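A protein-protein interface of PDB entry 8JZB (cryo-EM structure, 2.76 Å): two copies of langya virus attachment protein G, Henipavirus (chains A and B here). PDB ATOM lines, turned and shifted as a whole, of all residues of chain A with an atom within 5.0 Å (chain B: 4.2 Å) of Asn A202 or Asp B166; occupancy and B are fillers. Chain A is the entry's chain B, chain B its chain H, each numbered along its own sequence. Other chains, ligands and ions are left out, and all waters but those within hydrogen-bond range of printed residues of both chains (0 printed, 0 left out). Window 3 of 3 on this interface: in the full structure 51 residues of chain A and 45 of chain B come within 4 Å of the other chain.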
ATOM      1  N   GLY A 200       8.512  13.795 -13.472  1.00  0.00           N
ATOM      2  CA  GLY A 200       9.194  12.841 -12.630  1.00  0.00           C
ATOM      3  C   GLY A 200       8.364  12.457 -11.419  1.00  0.00           C
ATOM      4  O   GLY A 200       7.449  13.170 -11.014  1.00  0.00           O
ATOM      5  N   VAL A 201       8.694  11.303 -10.842  1.00  0.00           N
ATOM      6  CA  VAL A 201       7.936  10.804  -9.700  1.00  0.00           C
ATOM      7  C   VAL A 201       8.209  11.645  -8.458  1.00  0.00           C
ATOM      8  O   VAL A 201       7.302  11.914  -7.661  1.00  0.00           O
ATOM      9  CB  VAL A 201       8.254   9.318  -9.458  1.00  0.00           C
ATOM     10  CG1 VAL A 201       7.447   8.787  -8.285  1.00  0.00           C
ATOM     11  CG2 VAL A 201       7.979   8.509 -10.713  1.00  0.00           C
ATOM     12  N   ASN A 202       9.446  12.085  -8.274  1.00  0.00           N
ATOM     13  CA  ASN A 202       9.815  12.807  -7.060  1.00  0.00           C
ATOM     14  C   ASN A 202       9.757  14.329  -7.113  1.00  0.00           C
ATOM     15  O   ASN A 202       9.930  14.900  -8.170  1.00  0.00           O
ATOM     16  CB  ASN A 202      11.212  12.363  -6.669  1.00  0.00           C
ATOM     17  CG  ASN A 202      11.424  10.882  -6.843  1.00  0.00           C
ATOM     18  OD1 ASN A 202      12.163  10.455  -7.718  1.00  0.00           O
ATOM     19  ND2 ASN A 202      10.784  10.091  -6.001  1.00  0.00           N
ATOM     20  N   PHE A 203       9.542  14.978  -5.973  1.00  0.00           N
ATOM     21  CA  PHE A 203       9.433  16.429  -5.885  1.00  0.00           C
ATOM     22  C   PHE A 203      10.357  16.853  -4.777  1.00  0.00           C
ATOM     23  O   PHE A 203       9.908  17.150  -3.687  1.00  0.00           O
ATOM     24  CB  PHE A 203       8.009  16.814  -5.556  1.00  0.00           C
ATOM     25  CG  PHE A 203       7.593  18.162  -6.041  1.00  0.00           C
ATOM     26  CD1 PHE A 203       7.788  18.535  -7.349  1.00  0.00           C
ATOM     27  CD2 PHE A 203       6.962  19.043  -5.186  1.00  0.00           C
ATOM     28  CE1 PHE A 203       7.384  19.776  -7.792  1.00  0.00           C
ATOM     29  CE2 PHE A 203       6.556  20.281  -5.620  1.00  0.00           C
ATOM     30  CZ  PHE A 203       6.769  20.651  -6.927  1.00  0.00           C
ATOM     31  N   TYR A 204      11.648  16.858  -5.028  1.00  0.00           N
ATOM     32  CA  TYR A 204      12.641  17.171  -4.018  1.00  0.00           C
ATOM     33  C   TYR A 204      12.682  18.592  -3.506  1.00  0.00           C
ATOM     34  O   TYR A 204      12.351  19.505  -4.219  1.00  0.00           O
ATOM     35  CB  TYR A 204      14.011  16.836  -4.581  1.00  0.00           C
ATOM     36  CG  TYR A 204      14.126  15.546  -5.333  1.00  0.00           C
ATOM     37  CD1 TYR A 204      14.373  14.359  -4.669  1.00  0.00           C
ATOM     38  CD2 TYR A 204      14.038  15.521  -6.711  1.00  0.00           C
ATOM     39  CE1 TYR A 204      14.502  13.177  -5.355  1.00  0.00           C
ATOM     40  CE2 TYR A 204      14.164  14.344  -7.406  1.00  0.00           C
ATOM     41  CZ  TYR A 204      14.396  13.177  -6.719  1.00  0.00           C
ATOM     42  OH  TYR A 204      14.521  12.001  -7.410  1.00  0.00           O
ATOM     43  N   GLN A 264      20.079  14.672  -4.767  1.00  0.00           N
ATOM     44  CA  GLN A 264      19.548  14.223  -6.052  1.00  0.00           C
ATOM     45  C   GLN A 264      19.123  15.394  -6.929  1.00  0.00           C
ATOM     46  O   GLN A 264      19.414  15.415  -8.131  1.00  0.00           O
ATOM     47  CB  GLN A 264      18.375  13.271  -5.826  1.00  0.00           C
ATOM     48  CG  GLN A 264      18.723  12.055  -4.987  1.00  0.00           C
ATOM     49  CD  GLN A 264      17.987  12.033  -3.664  1.00  0.00           C
ATOM     50  OE1 GLN A 264      18.221  12.874  -2.798  1.00  0.00           O
ATOM     51  NE2 GLN A 264      17.091  11.067  -3.501  1.00  0.00           N
ATOM     52  N   SER A 597      11.889  20.852  -6.545  1.00  0.00           N
ATOM     53  CA  SER A 597      12.397  20.550  -7.885  1.00  0.00           C
ATOM     54  C   SER A 597      11.932  19.235  -8.478  1.00  0.00           C
ATOM     55  O   SER A 597      11.773  18.271  -7.768  1.00  0.00           O
ATOM     56  CB  SER A 597      13.917  20.538  -7.860  1.00  0.00           C
ATOM     57  OG  SER A 597      14.414  19.294  -7.424  1.00  0.00           O
ATOM     58  N   TYR A 598      11.660  19.201  -9.776  1.00  0.00           N
ATOM     59  CA  TYR A 598      11.261  17.973 -10.471  1.00  0.00           C
ATOM     60  C   TYR A 598      11.833  17.892 -11.877  1.00  0.00           C
ATOM     61  O   TYR A 598      12.361  18.855 -12.375  1.00  0.00           O
ATOM     62  CB  TYR A 598       9.745  17.850 -10.518  1.00  0.00           C
ATOM     63  CG  TYR A 598       9.015  18.895 -11.313  1.00  0.00           C
ATOM     64  CD1 TYR A 598       8.794  20.158 -10.795  1.00  0.00           C
ATOM     65  CD2 TYR A 598       8.509  18.604 -12.567  1.00  0.00           C
ATOM     66  CE1 TYR A 598       8.110  21.109 -11.515  1.00  0.00           C
ATOM     67  CE2 TYR A 598       7.824  19.548 -13.291  1.00  0.00           C
ATOM     68  CZ  TYR A 598       7.627  20.796 -12.758  1.00  0.00           C
ATOM     69  OH  TYR A 598       6.942  21.731 -13.483  1.00  0.00           O
ATOM     70  N   LYS B 162      14.950   4.085  -7.431  1.00  0.00           N
ATOM     71  CA  LYS B 162      13.636   3.575  -7.085  1.00  0.00           C
ATOM     72  C   LYS B 162      12.748   4.724  -6.624  1.00  0.00           C
ATOM     73  O   LYS B 162      13.197   5.570  -5.837  1.00  0.00           O
ATOM     74  CB  LYS B 162      13.734   2.507  -5.984  1.00  0.00           C
ATOM     75  CG  LYS B 162      12.431   1.771  -5.714  1.00  0.00           C
ATOM     76  CD  LYS B 162      12.566   0.806  -4.550  1.00  0.00           C
ATOM     77  CE  LYS B 162      11.372  -0.132  -4.479  1.00  0.00           C
ATOM     78  NZ  LYS B 162      10.086   0.613  -4.409  1.00  0.00           N
ATOM     79  N   PRO B 163      11.497   4.795  -7.084  1.00  0.00           N
ATOM     80  CA  PRO B 163      10.674   5.973  -6.758  1.00  0.00           C
ATOM     81  C   PRO B 163      10.161   5.999  -5.327  1.00  0.00           C
ATOM     82  O   PRO B 163      10.052   7.082  -4.742  1.00  0.00           O
ATOM     83  CB  PRO B 163       9.523   5.876  -7.770  1.00  0.00           C
ATOM     84  CG  PRO B 163       9.425   4.421  -8.079  1.00  0.00           C
ATOM     85  CD  PRO B 163      10.837   3.912  -8.061  1.00  0.00           C
ATOM     86  N   ASP B 164       9.837   4.843  -4.744  1.00  0.00           N
ATOM     87  CA  ASP B 164       9.156   4.832  -3.450  1.00  0.00           C
ATOM     88  C   ASP B 164      10.065   5.338  -2.334  1.00  0.00           C
ATOM     89  O   ASP B 164       9.671   6.202  -1.538  1.00  0.00           O
ATOM     90  CB  ASP B 164       8.649   3.424  -3.142  1.00  0.00           C
ATOM     91  CG  ASP B 164       7.758   2.875  -4.239  1.00  0.00           C
ATOM     92  OD1 ASP B 164       7.149   3.684  -4.969  1.00  0.00           O
ATOM     93  OD2 ASP B 164       7.669   1.637  -4.372  1.00  0.00           O
ATOM     94  N   ASP B 165      11.289   4.811  -2.257  1.00  0.00           N
ATOM     95  CA  ASP B 165      12.213   5.260  -1.221  1.00  0.00           C
ATOM     96  C   ASP B 165      12.568   6.730  -1.396  1.00  0.00           C
ATOM     97  O   ASP B 165      12.647   7.472  -0.409  1.00  0.00           O
ATOM     98  CB  ASP B 165      13.474   4.396  -1.229  1.00  0.00           C
ATOM     99  CG  ASP B 165      14.303   4.562   0.032  1.00  0.00           C
ATOM    100  OD1 ASP B 165      13.854   5.272   0.957  1.00  0.00           O
ATOM    101  OD2 ASP B 165      15.406   3.981   0.099  1.00  0.00           O
ATOM    102  N   ASP B 166      12.771   7.170  -2.641  1.00  0.00           N
ATOM    103  CA  ASP B 166      13.058   8.577  -2.889  1.00  0.00           C
ATOM    104  C   ASP B 166      11.902   9.462  -2.442  1.00  0.00           C
ATOM    105  O   ASP B 166      12.119  10.520  -1.841  1.00  0.00           O
ATOM    106  CB  ASP B 166      13.366   8.795  -4.369  1.00  0.00           C
ATOM    107  CG  ASP B 166      14.826   8.564  -4.699  1.00  0.00           C
ATOM    108  OD1 ASP B 166      15.692   9.018  -3.923  1.00  0.00           O
ATOM    109  OD2 ASP B 166      15.108   7.926  -5.736  1.00  0.00           O
ATOM    110  N   THR B 167      10.662   9.043  -2.716  1.00  0.00           N
ATOM    111  CA  THR B 167       9.507   9.804  -2.254  1.00  0.00           C
ATOM    112  C   THR B 167       9.456   9.852  -0.733  1.00  0.00           C
ATOM    113  O   THR B 167       9.067  10.871  -0.151  1.00  0.00           O
ATOM    114  CB  THR B 167       8.212   9.209  -2.808  1.00  0.00           C
ATOM    115  OG1 THR B 167       8.232   7.785  -2.652  1.00  0.00           O
ATOM    116  CG2 THR B 167       8.045   9.557  -4.277  1.00  0.00           C
ATOM    117  N   THR B 168       9.834   8.755  -0.073  1.00  0.00           N
ATOM    118  CA  THR B 168       9.913   8.789   1.385  1.00  0.00           C
ATOM    119  C   THR B 168      10.959   9.789   1.862  1.00  0.00           C
ATOM    120  O   THR B 168      10.741  10.479   2.864  1.00  0.00           O
ATOM    121  CB  THR B 168      10.217   7.401   1.949  1.00  0.00           C
ATOM    122  OG1 THR B 168      11.443   6.912   1.394  1.00  0.00           O
ATOM    123  CG2 THR B 168       9.090   6.434   1.621  1.00  0.00           C
ATOM    124  N   ASP B 169      12.093   9.884   1.168  1.00  0.00           N
ATOM    125  CA  ASP B 169      13.124  10.857   1.518  1.00  0.00           C
ATOM    126  C   ASP B 169      13.122  12.090   0.620  1.00  0.00           C
ATOM    127  O   ASP B 169      14.161  12.746   0.495  1.00  0.00           O
ATOM    128  CB  ASP B 169      14.511  10.196   1.499  1.00  0.00           C
ATOM    129  CG  ASP B 169      14.890   9.641   0.135  1.00  0.00           C
ATOM    130  OD1 ASP B 169      14.937  10.407  -0.850  1.00  0.00           O
ATOM    131  OD2 ASP B 169      15.167   8.426   0.052  1.00  0.00           O
ATOM    132  N   ASP B 170      12.003  12.477   0.046  1.00  0.00           N
ATOM    133  CA  ASP B 170      11.996  13.604  -0.863  1.00  0.00           C
ATOM    134  C   ASP B 170      12.210  14.939  -0.172  1.00  0.00           C
ATOM    135  O   ASP B 170      12.921  15.784  -0.689  1.00  0.00           O
ATOM    136  CB  ASP B 170      10.678  13.630  -1.613  1.00  0.00           C
ATOM    137  CG  ASP B 170      10.785  13.049  -3.001  1.00  0.00           C
ATOM    138  OD1 ASP B 170      11.891  12.630  -3.386  1.00  0.00           O
ATOM    139  OD2 ASP B 170       9.760  13.012  -3.709  1.00  0.00           O
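The side-chain carboxylate (OD2) of Asp B170 lies within hydrogen-bond range of the backbone NH (N) of Phe A203.
ND2 of Asn A202 sits at hydrogen-bond distance from O of Pro B163 (3.3 Å).
NE2 of Gln A264 is in hydrogen-bond range of OD1 of Asp B169 (3.5 Å).
The side-chain amide nitrogen (NE2) of Gln A264 sits at hydrogen-bond distance from the side-chain carboxylate (OD1) of Asp B166 (2.5 Å).
The backbone NH of Thr B167 sits close to the side-chain amide nitrogen of Asn A202 (3.5 Å).
The backbone carbonyl oxygen (O) of Pro B163 is in hydrogen-bond range of the side-chain hydroxyl (OG1) of Thr B167, at 2.9 Å.
The side-chain amide oxygen (OD1) of Asn A202 lies within hydrogen-bond range of the side-chain hydroxyl (OH) of Tyr A204 (2.8 Å).
The side-chain hydroxyl of Thr B167 is in hydrogen-bond range of the backbone carbonyl oxygen of Asp B164, 2.4 Å away.
The side-chain carboxylate of Asp B170 lies close to the backbone carbonyl oxygen of Asp B166, 2.6 Å away.
The backbone carbonyl oxygen (O) of Tyr A204 sits at hydrogen-bond distance from the backbone NH (N) of Ser A597 (2.7 Å).
The backbone carbonyl oxygen of Asp B165 sits close to the side-chain carboxylate of Asp B169 (2.7 Å).
Among the printed residues, merely in contact across the chains: Val A201 with Pro B163 (3.6 Å), Asn A202 with Asp B166 (3.3 Å), Asn A202 with Asp B170 (3.4 Å) and Tyr A204 with Asp B170 (3.3 Å).
Of chain B, only Pro B163 (3.3 Å), Asp B166 (3.3 Å), Thr B167 (3.3 Å) and Asp B170 (3.4 Å) come within 4 Å of Asn A202.
Of chain A, only Asn A202 (3.3 Å) and Gln A264 (2.5 Å) come within 4 Å of Asp B166.
Of the printed residues of chain B, Gln A264 touches Asp B166 and Asp B169.
Printed residues of chain A within 4 Å of Asp B170: Asn A202, Phe A203 and Tyr A204.
Of the printed residues of chain B, Tyr A204 touches Asp B170.
Of the printed residues of chain B, Phe A203 touches Asp B170.
Printed residues of chain B within 4 Å of Val A201: Pro B163.
The nearest residue of chain A that does not touch Asp B166 is Tyr A204 (4.4 Å).
The nearest printed residue of chain B that does not touch Phe A203 is Thr B167 (5.9 Å).
Printed residues of chain A that touch a printed residue of chain B: Val A201, Asn A202, Phe A203, Tyr A204 and Gln A264.
Hydrophobic or aromatic side chains of chain A within 4 Å of the printed part of chain B: Val A201 and Tyr A204.
Of the 9 printed residues of chain B, 5 touch a printed residue of chain A.
Among the printed residues, no Asp or Glu carboxylate lies within 4 Å of a Lys or Arg side-chain nitrogen of the other chain.
No position is printed for both chains.
Of the 9 pairs that touch across the chains among the printed residues, none has its exchanged pair printed and touching as well.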
